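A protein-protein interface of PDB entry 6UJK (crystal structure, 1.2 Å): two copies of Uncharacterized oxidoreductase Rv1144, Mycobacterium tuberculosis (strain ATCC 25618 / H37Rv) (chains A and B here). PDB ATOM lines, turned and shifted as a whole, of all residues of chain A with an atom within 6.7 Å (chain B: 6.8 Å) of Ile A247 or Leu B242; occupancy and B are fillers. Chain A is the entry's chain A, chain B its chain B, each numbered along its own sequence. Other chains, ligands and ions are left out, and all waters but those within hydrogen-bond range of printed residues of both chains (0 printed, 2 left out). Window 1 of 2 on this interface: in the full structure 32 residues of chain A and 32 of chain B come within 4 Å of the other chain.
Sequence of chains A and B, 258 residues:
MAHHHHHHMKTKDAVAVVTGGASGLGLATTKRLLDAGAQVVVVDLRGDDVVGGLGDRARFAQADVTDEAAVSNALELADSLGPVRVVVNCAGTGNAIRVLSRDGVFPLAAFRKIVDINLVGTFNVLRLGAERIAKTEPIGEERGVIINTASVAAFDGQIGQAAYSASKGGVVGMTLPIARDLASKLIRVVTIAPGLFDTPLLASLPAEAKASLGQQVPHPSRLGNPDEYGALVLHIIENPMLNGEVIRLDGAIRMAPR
OD2 of Asp A250 is in salt-bridge range of NE of Arg A248 (2.8 Å).
N of Val B189 sits at hydrogen-bond distance from OD1 of Asn B243 (2.9 Å).
The backbone carbonyl oxygen (O) of Val B189 is in hydrogen-bond range of the backbone NH (N) of Gly B244, at 2.8 Å.
The backbone carbonyl oxygen (O) of Ile B236 lies within hydrogen-bond range of the guanidinium group (NH1) of Arg B188, at 2.9 Å.
ND2 of Asn B239 lies within hydrogen-bond range of NE2 of His B235.
The backbone NH (N) of Thr A191 sits at hydrogen-bond distance from the backbone carbonyl oxygen (O) of Glu A245, at 3.0 Å.
Of the 19 printed residues of chain A, 12 touch a printed residue of chain B.
Hydrophobic or aromatic side chains of chain A within 4 Å of the printed part of chain B: His A219, Pro A220, Leu A232, Leu A242, Ile A247, Leu A249 and Ala A252.
Along chain A the printed residues that touch a printed residue of chain B span positions 219 to 252.
Of the 18 printed residues of chain B, 12 touch a printed residue of chain A.
Hydrophobic or aromatic side chains of chain B that line the printed part of chain A: His B235, Met B241, Leu B242 and Ile B247.
Among the printed residues, no Asp or Glu carboxylate lies within 4 Å of a Lys or Arg side-chain nitrogen of the other chain.
Among the printed residues, pairs that only touch across the chains: His A219 with Arg B188, Pro A220 with Pro B240, Pro A220 with Met B241, Leu A232 with His B235, Leu A232 with Asn B239, Leu A242 with Ile B247, Leu A242 with Arg B248, Glu A245 with Val B246, Glu A245 with Ile B247, Val A246 with Glu B245, Ile A247 with Leu B242, Ile A247 with Glu B245, Arg A248 with Leu B242, Leu A249 with Asn B239, Leu A249 with Met B241, Leu A249 with Leu B242, Asp A250 with Asn B243, Gly A251 with Asn B243 and Ala A252 with Gly B244.
N of Asp A250 is in hydrogen-bond range of O of Met B241, at 3.3 Å.
The backbone NH (N) of Ala A252 lies within hydrogen-bond range of the backbone carbonyl oxygen (O) of Asn B243 (3.2 Å).
The backbone NH (N) of Gly A251 is in hydrogen-bond range of the backbone carbonyl oxygen (O) of Met B241 (2.9 Å).
The backbone NH of Arg B248 is in hydrogen-bond range of the side-chain carboxylate of Glu A245 (2.8 Å).
The backbone carbonyl oxygen of His A219 is in hydrogen-bond range of the side-chain amide nitrogen of Asn B243 (2.9 Å).
OE2 of Glu B245 lies within hydrogen-bond range of N of Arg A248 (2.8 Å).
Ile A192 touches none of the printed residues of chain B.
Ile A236 touches none of the printed residues of chain B.
Ile A247 touches two residues of chain B.
Of the printed residues of chain A, Asn B239 touches Leu A232 and Leu A249.
Printed residues of chain A within 4 Å of Pro B240: Pro A220.
Of chain A, only Ile A247 (3.9 Å), Arg A248 (3.6 Å) and Leu A249 (3.6 Å) come within 4 Å of Leu B242.
Printed residues of chain A within 4 Å of Ile B247: Leu A242 and Glu A245.
The nearest residue of chain B that does not touch Ile A247 is Ile B247 (4.1 Å).
The nearest residue of chain A that does not touch Leu B242 is Leu A232 (4.6 Å).
The nearest printed residue of chain B that does not touch Glu A245 is Glu B245 (5.3 Å).
Leu A242 touches Ile B247, and with the chains exchanged Ile A247 touches Leu B242.
Leu A242 touches Arg B248, and with the chains exchanged Arg A248 touches Leu B242.
Glu A245 touches Ile B247, and with the chains exchanged Ile A247 touches Glu B245.
Glu A245 touches Arg B248, and with the chains exchanged Arg A248 touches Glu B245.
Of the 25 pairs that touch across the chains among the printed residues, 10 have their exchanged pair printed and touching as well.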
ATOM      1  N   PHE A 155     -21.682 -27.775 -29.211  1.00  0.00           N
ATOM      2  CA  PHE A 155     -21.399 -29.204 -29.152  1.00  0.00           C
ATOM      3  C   PHE A 155     -22.103 -29.993 -30.241  1.00  0.00           C
ATOM      4  O   PHE A 155     -21.570 -31.013 -30.682  1.00  0.00           O
ATOM      5  CB  PHE A 155     -21.855 -29.759 -27.793  1.00  0.00           C
ATOM      6  CG  PHE A 155     -21.306 -28.981 -26.626  1.00  0.00           C
ATOM      7  CD1 PHE A 155     -19.945 -28.996 -26.346  1.00  0.00           C
ATOM      8  CD2 PHE A 155     -22.133 -28.218 -25.809  1.00  0.00           C
ATOM      9  CE1 PHE A 155     -19.437 -28.276 -25.273  1.00  0.00           C
ATOM     10  CE2 PHE A 155     -21.619 -27.486 -24.721  1.00  0.00           C
ATOM     11  CZ  PHE A 155     -20.271 -27.527 -24.465  1.00  0.00           C
ATOM     12  N   VAL A 190     -19.074 -18.621 -15.414  1.00  0.00           N
ATOM     13  CA  VAL A 190     -19.828 -19.824 -15.737  1.00  0.00           C
ATOM     14  C   VAL A 190     -20.567 -19.557 -17.035  1.00  0.00           C
ATOM     15  O   VAL A 190     -20.984 -18.419 -17.290  1.00  0.00           O
ATOM     16  CB  VAL A 190     -20.818 -20.188 -14.596  1.00  0.00           C
ATOM     17  CG1 VAL A 190     -21.681 -21.412 -14.960  1.00  0.00           C
ATOM     18  CG2 VAL A 190     -20.055 -20.450 -13.308  1.00  0.00           C
ATOM     19  N   THR A 191     -20.775 -20.605 -17.828  1.00  0.00           N
ATOM     20  CA  THR A 191     -21.467 -20.474 -19.101  1.00  0.00           C
ATOM     21  C   THR A 191     -22.648 -21.428 -19.125  1.00  0.00           C
ATOM     22  O   THR A 191     -22.526 -22.593 -18.728  1.00  0.00           O
ATOM     23  CB  THR A 191     -20.482 -20.720 -20.228  1.00  0.00           C
ATOM     24  OG1 THR A 191     -19.545 -19.634 -20.217  1.00  0.00           O
ATOM     25  CG2 THR A 191     -21.133 -20.835 -21.595  1.00  0.00           C
ATOM     26  N   ILE A 192     -23.790 -20.942 -19.596  1.00  0.00           N
ATOM     27  CA  ILE A 192     -24.952 -21.776 -19.825  1.00  0.00           C
ATOM     28  C   ILE A 192     -25.049 -22.041 -21.316  1.00  0.00           C
ATOM     29  O   ILE A 192     -24.903 -21.113 -22.130  1.00  0.00           O
ATOM     30  CB  ILE A 192     -26.231 -21.077 -19.334  1.00  0.00           C
ATOM     31  CG1 ILE A 192     -26.159 -20.774 -17.838  1.00  0.00           C
ATOM     32  CG2 ILE A 192     -27.450 -21.940 -19.638  1.00  0.00           C
ATOM     33  CD1 ILE A 192     -27.242 -19.809 -17.375  1.00  0.00           C
ATOM     34  N   ALA A 193     -25.335 -23.296 -21.683  1.00  0.00           N
ATOM     35  CA  ALA A 193     -25.547 -23.689 -23.075  1.00  0.00           C
ATOM     36  C   ALA A 193     -27.015 -24.052 -23.265  1.00  0.00           C
ATOM     37  O   ALA A 193     -27.416 -25.208 -23.051  1.00  0.00           O
ATOM     38  CB  ALA A 193     -24.626 -24.858 -23.432  1.00  0.00           C
ATOM     39  N   PRO A 194     -27.869 -23.101 -23.644  1.00  0.00           N
ATOM     40  CA  PRO A 194     -29.293 -23.429 -23.796  1.00  0.00           C
ATOM     41  C   PRO A 194     -29.554 -24.282 -25.018  1.00  0.00           C
ATOM     42  O   PRO A 194     -28.865 -24.170 -26.041  1.00  0.00           O
ATOM     43  CB  PRO A 194     -29.970 -22.059 -23.960  1.00  0.00           C
ATOM     44  CG  PRO A 194     -29.016 -21.066 -23.483  1.00  0.00           C
ATOM     45  CD  PRO A 194     -27.648 -21.651 -23.797  1.00  0.00           C
ATOM     46  N   HIS A 219     -37.492 -34.471 -22.814  1.00  0.00           N
ATOM     47  CA  HIS A 219     -38.357 -34.184 -21.675  1.00  0.00           C
ATOM     48  C   HIS A 219     -37.760 -33.005 -20.930  1.00  0.00           C
ATOM     49  O   HIS A 219     -36.597 -33.075 -20.512  1.00  0.00           O
ATOM     50  CB  HIS A 219     -38.497 -35.402 -20.755  1.00  0.00           C
ATOM     51  CG  HIS A 219     -39.242 -35.119 -19.491  1.00  0.00           C
ATOM     52  ND1 HIS A 219     -40.507 -34.561 -19.452  1.00  0.00           N
ATOM     53  CD2 HIS A 219     -38.871 -35.324 -18.205  1.00  0.00           C
ATOM     54  CE1 HIS A 219     -40.866 -34.427 -18.184  1.00  0.00           C
ATOM     55  NE2 HIS A 219     -39.899 -34.888 -17.408  1.00  0.00           N
ATOM     56  N   PRO A 220     -38.513 -31.917 -20.715  1.00  0.00           N
ATOM     57  CA  PRO A 220     -39.908 -31.747 -21.145  1.00  0.00           C
ATOM     58  C   PRO A 220     -39.998 -31.510 -22.648  1.00  0.00           C
ATOM     59  O   PRO A 220     -39.175 -30.820 -23.251  1.00  0.00           O
ATOM     60  CB  PRO A 220     -40.354 -30.515 -20.369  1.00  0.00           C
ATOM     61  CG  PRO A 220     -39.120 -29.692 -20.285  1.00  0.00           C
ATOM     62  CD  PRO A 220     -37.971 -30.668 -20.142  1.00  0.00           C
ATOM     63  N   LEU A 232     -31.712 -20.556 -13.660  1.00  0.00           N
ATOM     64  CA  LEU A 232     -30.371 -21.113 -13.578  1.00  0.00           C
ATOM     65  C   LEU A 232     -29.336 -20.017 -13.348  1.00  0.00           C
ATOM     66  O   LEU A 232     -28.391 -20.213 -12.572  1.00  0.00           O
ATOM     67  CB  LEU A 232     -30.067 -21.932 -14.831  1.00  0.00           C
ATOM     68  CG  LEU A 232     -28.671 -22.574 -14.862  1.00  0.00           C
ATOM     69  CD1 LEU A 232     -28.405 -23.481 -13.651  1.00  0.00           C
ATOM     70  CD2 LEU A 232     -28.503 -23.339 -16.158  1.00  0.00           C
ATOM     71  N   ILE A 236     -26.660 -20.040 -10.220  1.00  0.00           N
ATOM     72  CA  ILE A 236     -25.224 -19.851 -10.352  1.00  0.00           C
ATOM     73  C   ILE A 236     -24.758 -18.732  -9.441  1.00  0.00           C
ATOM     74  O   ILE A 236     -23.727 -18.848  -8.763  1.00  0.00           O
ATOM     75  CB  ILE A 236     -24.842 -19.587 -11.818  1.00  0.00           C
ATOM     76  CG1 ILE A 236     -25.106 -20.822 -12.682  1.00  0.00           C
ATOM     77  CG2 ILE A 236     -23.405 -19.125 -11.924  1.00  0.00           C
ATOM     78  CD1 ILE A 236     -25.194 -20.518 -14.178  1.00  0.00           C
ATOM     79  N   LEU A 242     -20.042 -23.220  -8.163  1.00  0.00           N
ATOM     80  CA  LEU A 242     -20.125 -23.328  -9.617  1.00  0.00           C
ATOM     81  C   LEU A 242     -19.145 -22.347 -10.265  1.00  0.00           C
ATOM     82  O   LEU A 242     -19.292 -21.120 -10.128  1.00  0.00           O
ATOM     83  CB  LEU A 242     -21.541 -23.057 -10.096  1.00  0.00           C
ATOM     84  CG  LEU A 242     -22.540 -24.189  -9.832  1.00  0.00           C
ATOM     85  CD1 LEU A 242     -23.968 -23.747 -10.096  1.00  0.00           C
ATOM     86  CD2 LEU A 242     -22.202 -25.407 -10.689  1.00  0.00           C
ATOM     87  N   GLU A 245     -17.319 -23.799 -15.559  1.00  0.00           N
ATOM     88  CA  GLU A 245     -18.102 -24.889 -16.107  1.00  0.00           C
ATOM     89  C   GLU A 245     -19.096 -24.357 -17.122  1.00  0.00           C
ATOM     90  O   GLU A 245     -19.498 -23.185 -17.069  1.00  0.00           O
ATOM     91  CB  GLU A 245     -18.820 -25.602 -14.940  1.00  0.00           C
ATOM     92  CG  GLU A 245     -19.860 -26.649 -15.248  1.00  0.00           C
ATOM     93  CD  GLU A 245     -19.391 -27.844 -16.079  1.00  0.00           C
ATOM     94  OE1 GLU A 245     -18.485 -27.707 -16.938  1.00  0.00           O
ATOM     95  OE2 GLU A 245     -20.010 -28.926 -15.929  1.00  0.00           O
ATOM     96  N   VAL A 246     -19.489 -25.250 -18.023  1.00  0.00           N
ATOM     97  CA  VAL A 246     -20.564 -25.032 -18.985  1.00  0.00           C
ATOM     98  C   VAL A 246     -21.703 -25.977 -18.622  1.00  0.00           C
ATOM     99  O   VAL A 246     -21.478 -27.179 -18.444  1.00  0.00           O
ATOM    100  CB  VAL A 246     -20.088 -25.292 -20.425  1.00  0.00           C
ATOM    101  CG1 VAL A 246     -21.250 -25.174 -21.423  1.00  0.00           C
ATOM    102  CG2 VAL A 246     -18.917 -24.377 -20.794  1.00  0.00           C
ATOM    103  N   ILE A 247     -22.921 -25.449 -18.522  1.00  0.00           N
ATOM    104  CA  ILE A 247     -24.092 -26.234 -18.140  1.00  0.00           C
ATOM    105  C   ILE A 247     -25.075 -26.246 -19.306  1.00  0.00           C
ATOM    106  O   ILE A 247     -25.608 -25.192 -19.674  1.00  0.00           O
ATOM    107  CB  ILE A 247     -24.780 -25.652 -16.892  1.00  0.00           C
ATOM    108  CG1 ILE A 247     -23.786 -25.548 -15.727  1.00  0.00           C
ATOM    109  CG2 ILE A 247     -26.011 -26.488 -16.527  1.00  0.00           C
ATOM    110  CD1 ILE A 247     -24.325 -24.853 -14.497  1.00  0.00           C
ATOM    111  N   ARG A 248     -25.374 -27.437 -19.852  1.00  0.00           N
ATOM    112  CA  ARG A 248     -26.426 -27.573 -20.855  1.00  0.00           C
ATOM    113  C   ARG A 248     -27.794 -27.484 -20.181  1.00  0.00           C
ATOM    114  O   ARG A 248     -28.044 -28.167 -19.172  1.00  0.00           O
ATOM    115  CB  ARG A 248     -26.321 -28.921 -21.573  1.00  0.00           C
ATOM    116  CG  ARG A 248     -25.050 -29.099 -22.398  1.00  0.00           C
ATOM    117  CD  ARG A 248     -24.952 -30.485 -23.065  1.00  0.00           C
ATOM    118  NE  ARG A 248     -26.019 -30.650 -24.046  1.00  0.00           N
ATOM    119  CZ  ARG A 248     -25.891 -30.871 -25.357  1.00  0.00           C
ATOM    120  NH1 ARG A 248     -24.693 -31.057 -25.930  1.00  0.00           N
ATOM    121  NH2 ARG A 248     -26.977 -30.862 -26.107  1.00  0.00           N
ATOM    122  N   LEU A 249     -28.687 -26.671 -20.760  1.00  0.00           N
ATOM    123  CA  LEU A 249     -30.034 -26.435 -20.229  1.00  0.00           C
ATOM    124  C   LEU A 249     -30.958 -26.700 -21.416  1.00  0.00           C
ATOM    125  O   LEU A 249     -31.244 -25.784 -22.207  1.00  0.00           O
ATOM    126  CB  LEU A 249     -30.165 -25.028 -19.684  1.00  0.00           C
ATOM    127  CG  LEU A 249     -31.517 -24.699 -19.064  1.00  0.00           C
ATOM    128  CD1 LEU A 249     -31.764 -25.521 -17.795  1.00  0.00           C
ATOM    129  CD2 LEU A 249     -31.622 -23.207 -18.777  1.00  0.00           C
ATOM    130  N   ASP A 250     -31.390 -27.966 -21.583  1.00  0.00           N
ATOM    131  CA  ASP A 250     -31.825 -28.401 -22.903  1.00  0.00           C
ATOM    132  C   ASP A 250     -32.800 -29.571 -22.947  1.00  0.00           C
ATOM    133  O   ASP A 250     -33.050 -30.078 -24.039  1.00  0.00           O
ATOM    134  CB  ASP A 250     -30.604 -28.691 -23.783  1.00  0.00           C
ATOM    135  CG  ASP A 250     -29.812 -29.904 -23.301  1.00  0.00           C
ATOM    136  OD1 ASP A 250     -30.258 -30.595 -22.328  1.00  0.00           O
ATOM    137  OD2 ASP A 250     -28.745 -30.156 -23.892  1.00  0.00           O
ATOM    138  N   GLY A 251     -33.381 -30.002 -21.820  1.00  0.00           N
ATOM    139  CA  GLY A 251     -34.353 -31.077 -21.907  1.00  0.00           C
ATOM    140  C   GLY A 251     -33.804 -32.385 -22.440  1.00  0.00           C
ATOM    141  O   GLY A 251     -34.572 -33.239 -22.913  1.00  0.00           O
ATOM    142  N   ALA A 252     -32.485 -32.564 -22.358  1.00  0.00           N
ATOM    143  CA  ALA A 252     -31.753 -33.743 -22.816  1.00  0.00           C
ATOM    144  C   ALA A 252     -31.670 -33.851 -24.336  1.00  0.00           C
ATOM    145  O   ALA A 252     -31.285 -34.914 -24.838  1.00  0.00           O
ATOM    146  CB  ALA A 252     -32.239 -35.061 -22.207  1.00  0.00           C
ATOM    147  N   VAL B 145     -37.706 -36.893 -10.686  1.00  0.00           N
ATOM    148  CA  VAL B 145     -36.321 -36.561 -11.039  1.00  0.00           C
ATOM    149  C   VAL B 145     -35.409 -37.526 -10.293  1.00  0.00           C
ATOM    150  O   VAL B 145     -35.611 -37.754  -9.087  1.00  0.00           O
ATOM    151  CB  VAL B 145     -35.978 -35.119 -10.596  1.00  0.00           C
ATOM    152  CG1 VAL B 145     -34.570 -34.740 -11.038  1.00  0.00           C
ATOM    153  CG2 VAL B 145     -36.993 -34.098 -11.106  1.00  0.00           C
ATOM    154  N   ARG B 188     -36.885 -36.976 -15.228  1.00  0.00           N
ATOM    155  CA  ARG B 188     -35.588 -36.426 -15.604  1.00  0.00           C
ATOM    156  C   ARG B 188     -34.474 -37.162 -14.881  1.00  0.00           C
ATOM    157  O   ARG B 188     -34.674 -37.712 -13.790  1.00  0.00           O
ATOM    158  CB  ARG B 188     -35.525 -34.928 -15.281  1.00  0.00           C
ATOM    159  CG  ARG B 188     -36.427 -34.110 -16.160  1.00  0.00           C
ATOM    160  CD  ARG B 188     -36.321 -32.622 -15.932  1.00  0.00           C
ATOM    161  NE  ARG B 188     -36.865 -32.189 -14.647  1.00  0.00           N
ATOM    162  CZ  ARG B 188     -36.192 -31.584 -13.663  1.00  0.00           C
ATOM    163  NH1 ARG B 188     -34.884 -31.366 -13.727  1.00  0.00           N
ATOM    164  NH2 ARG B 188     -36.870 -31.214 -12.592  1.00  0.00           N
ATOM    165  N   VAL B 189     -33.284 -37.163 -15.494  1.00  0.00           N
ATOM    166  CA  VAL B 189     -32.109 -37.816 -14.920  1.00  0.00           C
ATOM    167  C   VAL B 189     -30.932 -36.871 -15.130  1.00  0.00           C
ATOM    168  O   VAL B 189     -30.609 -36.518 -16.271  1.00  0.00           O
ATOM    169  CB  VAL B 189     -31.840 -39.172 -15.585  1.00  0.00           C
ATOM    170  CG1 VAL B 189     -30.640 -39.851 -14.935  1.00  0.00           C
ATOM    171  CG2 VAL B 189     -33.074 -40.064 -15.505  1.00  0.00           C
ATOM    172  N   VAL B 190     -30.299 -36.433 -14.038  1.00  0.00           N
ATOM    173  CA  VAL B 190     -29.193 -35.474 -14.072  1.00  0.00           C
ATOM    174  C   VAL B 190     -28.096 -35.981 -13.147  1.00  0.00           C
ATOM    175  O   VAL B 190     -28.388 -36.614 -12.121  1.00  0.00           O
ATOM    176  CB  VAL B 190     -29.670 -34.069 -13.629  1.00  0.00           C
ATOM    177  CG1 VAL B 190     -28.517 -33.066 -13.576  1.00  0.00           C
ATOM    178  CG2 VAL B 190     -30.775 -33.557 -14.533  1.00  0.00           C
ATOM    179  N   LEU B 232     -27.547 -27.412  -5.188  1.00  0.00           N
ATOM    180  CA  LEU B 232     -27.655 -27.751  -6.602  1.00  0.00           C
ATOM    181  C   LEU B 232     -28.693 -28.843  -6.836  1.00  0.00           C
ATOM    182  O   LEU B 232     -29.446 -28.788  -7.820  1.00  0.00           O
ATOM    183  CB  LEU B 232     -26.288 -28.144  -7.169  1.00  0.00           C
ATOM    184  CG  LEU B 232     -26.262 -28.528  -8.650  1.00  0.00           C
ATOM    185  CD1 LEU B 232     -26.811 -27.424  -9.559  1.00  0.00           C
ATOM    186  CD2 LEU B 232     -24.847 -28.898  -9.066  1.00  0.00           C
ATOM    187  N   HIS B 235     -31.956 -27.134  -6.907  1.00  0.00           N
ATOM    188  CA  HIS B 235     -32.177 -26.393  -8.138  1.00  0.00           C
ATOM    189  C   HIS B 235     -32.551 -27.331  -9.283  1.00  0.00           C
ATOM    190  O   HIS B 235     -33.438 -27.019 -10.086  1.00  0.00           O
ATOM    191  CB  HIS B 235     -30.989 -25.537  -8.523  1.00  0.00           C
ATOM    192  CG  HIS B 235     -31.311 -24.715  -9.725  1.00  0.00           C
ATOM    193  ND1 HIS B 235     -32.283 -23.741  -9.698  1.00  0.00           N
ATOM    194  CD2 HIS B 235     -30.911 -24.799 -11.023  1.00  0.00           C
ATOM    195  CE1 HIS B 235     -32.440 -23.242 -10.916  1.00  0.00           C
ATOM    196  NE2 HIS B 235     -31.624 -23.866 -11.742  1.00  0.00           N
ATOM    197  N   ILE B 236     -31.867 -28.484  -9.394  1.00  0.00           N
ATOM    198  CA  ILE B 236     -32.220 -29.442 -10.434  1.00  0.00           C
ATOM    199  C   ILE B 236     -33.679 -29.855 -10.289  1.00  0.00           C
ATOM    200  O   ILE B 236     -34.418 -29.944 -11.281  1.00  0.00           O
ATOM    201  CB  ILE B 236     -31.275 -30.656 -10.387  1.00  0.00           C
ATOM    202  CG1 ILE B 236     -29.848 -30.250 -10.786  1.00  0.00           C
ATOM    203  CG2 ILE B 236     -31.806 -31.789 -11.267  1.00  0.00           C
ATOM    204  CD1 ILE B 236     -28.791 -31.248 -10.337  1.00  0.00           C
ATOM    205  N   ILE B 237     -34.122 -30.134  -9.055  1.00  0.00           N
ATOM    206  CA  ILE B 237     -35.514 -30.520  -8.846  1.00  0.00           C
ATOM    207  C   ILE B 237     -36.449 -29.433  -9.339  1.00  0.00           C
ATOM    208  O   ILE B 237     -37.473 -29.714  -9.972  1.00  0.00           O
ATOM    209  CB  ILE B 237     -35.750 -30.846  -7.360  1.00  0.00           C
ATOM    210  CG1 ILE B 237     -34.967 -32.109  -6.967  1.00  0.00           C
ATOM    211  CG2 ILE B 237     -37.251 -31.015  -7.089  1.00  0.00           C
ATOM    212  CD1 ILE B 237     -34.839 -32.316  -5.476  1.00  0.00           C
ATOM    213  N   ASN B 239     -35.888 -26.963 -11.598  1.00  0.00           N
ATOM    214  CA  ASN B 239     -35.681 -26.420 -12.937  1.00  0.00           C
ATOM    215  C   ASN B 239     -36.038 -27.493 -13.953  1.00  0.00           C
ATOM    216  O   ASN B 239     -35.226 -28.399 -14.211  1.00  0.00           O
ATOM    217  CB  ASN B 239     -34.247 -25.934 -13.145  1.00  0.00           C
ATOM    218  CG  ASN B 239     -34.128 -25.122 -14.409  1.00  0.00           C
ATOM    219  OD1 ASN B 239     -34.854 -25.364 -15.385  1.00  0.00           O
ATOM    220  ND2 ASN B 239     -33.251 -24.132 -14.398  1.00  0.00           N
ATOM    221  N   PRO B 240     -37.223 -27.426 -14.574  1.00  0.00           N
ATOM    222  CA  PRO B 240     -37.664 -28.525 -15.448  1.00  0.00           C
ATOM    223  C   PRO B 240     -36.783 -28.752 -16.659  1.00  0.00           C
ATOM    224  O   PRO B 240     -36.844 -29.837 -17.248  1.00  0.00           O
ATOM    225  CB  PRO B 240     -39.082 -28.104 -15.880  1.00  0.00           C
ATOM    226  CG  PRO B 240     -39.545 -27.175 -14.864  1.00  0.00           C
ATOM    227  CD  PRO B 240     -38.303 -26.451 -14.355  1.00  0.00           C
ATOM    228  N   MET B 241     -35.986 -27.768 -17.089  1.00  0.00           N
ATOM    229  CA  MET B 241     -35.203 -27.939 -18.306  1.00  0.00           C
ATOM    230  C   MET B 241     -33.885 -28.663 -18.100  1.00  0.00           C
ATOM    231  O   MET B 241     -33.240 -28.987 -19.096  1.00  0.00           O
ATOM    232  CB  MET B 241     -34.989 -26.590 -18.987  1.00  0.00           C
ATOM    233  CG  MET B 241     -36.221 -26.120 -19.712  1.00  0.00           C
ATOM    234  SD  MET B 241     -36.546 -27.080 -21.194  1.00  0.00           S
ATOM    235  CE  MET B 241     -35.115 -26.667 -22.196  1.00  0.00           C
ATOM    236  N   LEU B 242     -33.440 -28.903 -16.866  1.00  0.00           N
ATOM    237  CA  LEU B 242     -32.190 -29.633 -16.660  1.00  0.00           C
ATOM    238  C   LEU B 242     -32.436 -31.128 -16.802  1.00  0.00           C
ATOM    239  O   LEU B 242     -33.171 -31.716 -15.996  1.00  0.00           O
ATOM    240  CB  LEU B 242     -31.607 -29.319 -15.292  1.00  0.00           C
ATOM    241  CG  LEU B 242     -30.944 -27.942 -15.171  1.00  0.00           C
ATOM    242  CD1 LEU B 242     -30.640 -27.587 -13.730  1.00  0.00           C
ATOM    243  CD2 LEU B 242     -29.671 -27.837 -16.025  1.00  0.00           C
ATOM    244  N   ASN B 243     -31.824 -31.751 -17.806  1.00  0.00           N
ATOM    245  CA  ASN B 243     -32.074 -33.165 -18.045  1.00  0.00           C
ATOM    246  C   ASN B 243     -30.954 -33.721 -18.913  1.00  0.00           C
ATOM    247  O   ASN B 243     -30.508 -33.059 -19.851  1.00  0.00           O
ATOM    248  CB  ASN B 243     -33.441 -33.381 -18.722  1.00  0.00           C
ATOM    249  CG  ASN B 243     -33.892 -34.829 -18.678  1.00  0.00           C
ATOM    250  OD1 ASN B 243     -33.337 -35.636 -17.924  1.00  0.00           O
ATOM    251  ND2 ASN B 243     -34.886 -35.180 -19.496  1.00  0.00           N
ATOM    252  N   GLY B 244     -30.501 -34.936 -18.597  1.00  0.00           N
ATOM    253  CA  GLY B 244     -29.542 -35.619 -19.444  1.00  0.00           C
ATOM    254  C   GLY B 244     -28.161 -35.042 -19.428  1.00  0.00           C
ATOM    255  O   GLY B 244     -27.374 -35.328 -20.348  1.00  0.00           O
ATOM    256  N   GLU B 245     -27.825 -34.265 -18.394  1.00  0.00           N
ATOM    257  CA  GLU B 245     -26.611 -33.469 -18.318  1.00  0.00           C
ATOM    258  C   GLU B 245     -25.818 -33.838 -17.073  1.00  0.00           C
ATOM    259  O   GLU B 245     -26.378 -34.329 -16.085  1.00  0.00           O
ATOM    260  CB  GLU B 245     -27.009 -31.973 -18.317  1.00  0.00           C
ATOM    261  CG  GLU B 245     -25.920 -30.943 -18.018  1.00  0.00           C
ATOM    262  CD  GLU B 245     -24.723 -30.917 -18.970  1.00  0.00           C
ATOM    263  OE1 GLU B 245     -24.344 -31.981 -19.506  1.00  0.00           O
ATOM    264  OE2 GLU B 245     -24.120 -29.819 -19.119  1.00  0.00           O
ATOM    265  N   VAL B 246     -24.509 -33.596 -17.153  1.00  0.00           N
ATOM    266  CA  VAL B 246     -23.592 -33.721 -16.028  1.00  0.00           C
ATOM    267  C   VAL B 246     -23.092 -32.324 -15.706  1.00  0.00           C
ATOM    268  O   VAL B 246     -22.660 -31.607 -16.606  1.00  0.00           O
ATOM    269  CB  VAL B 246     -22.406 -34.641 -16.385  1.00  0.00           C
ATOM    270  CG1 VAL B 246     -21.413 -34.669 -15.257  1.00  0.00           C
ATOM    271  CG2 VAL B 246     -22.908 -36.025 -16.757  1.00  0.00           C
ATOM    272  N   ILE B 247     -23.143 -31.939 -14.436  1.00  0.00           N
ATOM    273  CA  ILE B 247     -22.744 -30.600 -13.989  1.00  0.00           C
ATOM    274  C   ILE B 247     -21.556 -30.729 -13.050  1.00  0.00           C
ATOM    275  O   ILE B 247     -21.680 -31.326 -11.971  1.00  0.00           O
ATOM    276  CB  ILE B 247     -23.898 -29.875 -13.281  1.00  0.00           C
ATOM    277  CG1 ILE B 247     -25.135 -29.800 -14.172  1.00  0.00           C
ATOM    278  CG2 ILE B 247     -23.457 -28.516 -12.803  1.00  0.00           C
ATOM    279  CD1 ILE B 247     -26.342 -29.232 -13.486  1.00  0.00           C
ATOM    280  N   ARG B 248     -20.412 -30.159 -13.435  1.00  0.00           N
ATOM    281  CA  ARG B 248     -19.258 -30.104 -12.529  1.00  0.00           C
ATOM    282  C   ARG B 248     -19.504 -29.031 -11.469  1.00  0.00           C
ATOM    283  O   ARG B 248     -19.888 -27.893 -11.795  1.00  0.00           O
ATOM    284  CB  ARG B 248     -17.988 -29.731 -13.299  1.00  0.00           C
ATOM    285  CG  ARG B 248     -17.526 -30.789 -14.310  1.00  0.00           C
ATOM    286  CD  ARG B 248     -16.269 -30.369 -15.097  1.00  0.00           C
ATOM    287  NE  ARG B 248     -15.132 -30.245 -14.187  1.00  0.00           N
ATOM    288  CZ  ARG B 248     -13.992 -30.940 -14.232  1.00  0.00           C
ATOM    289  NH1 ARG B 248     -13.696 -31.789 -15.221  1.00  0.00           N
ATOM    290  NH2 ARG B 248     -13.121 -30.782 -13.265  1.00  0.00           N
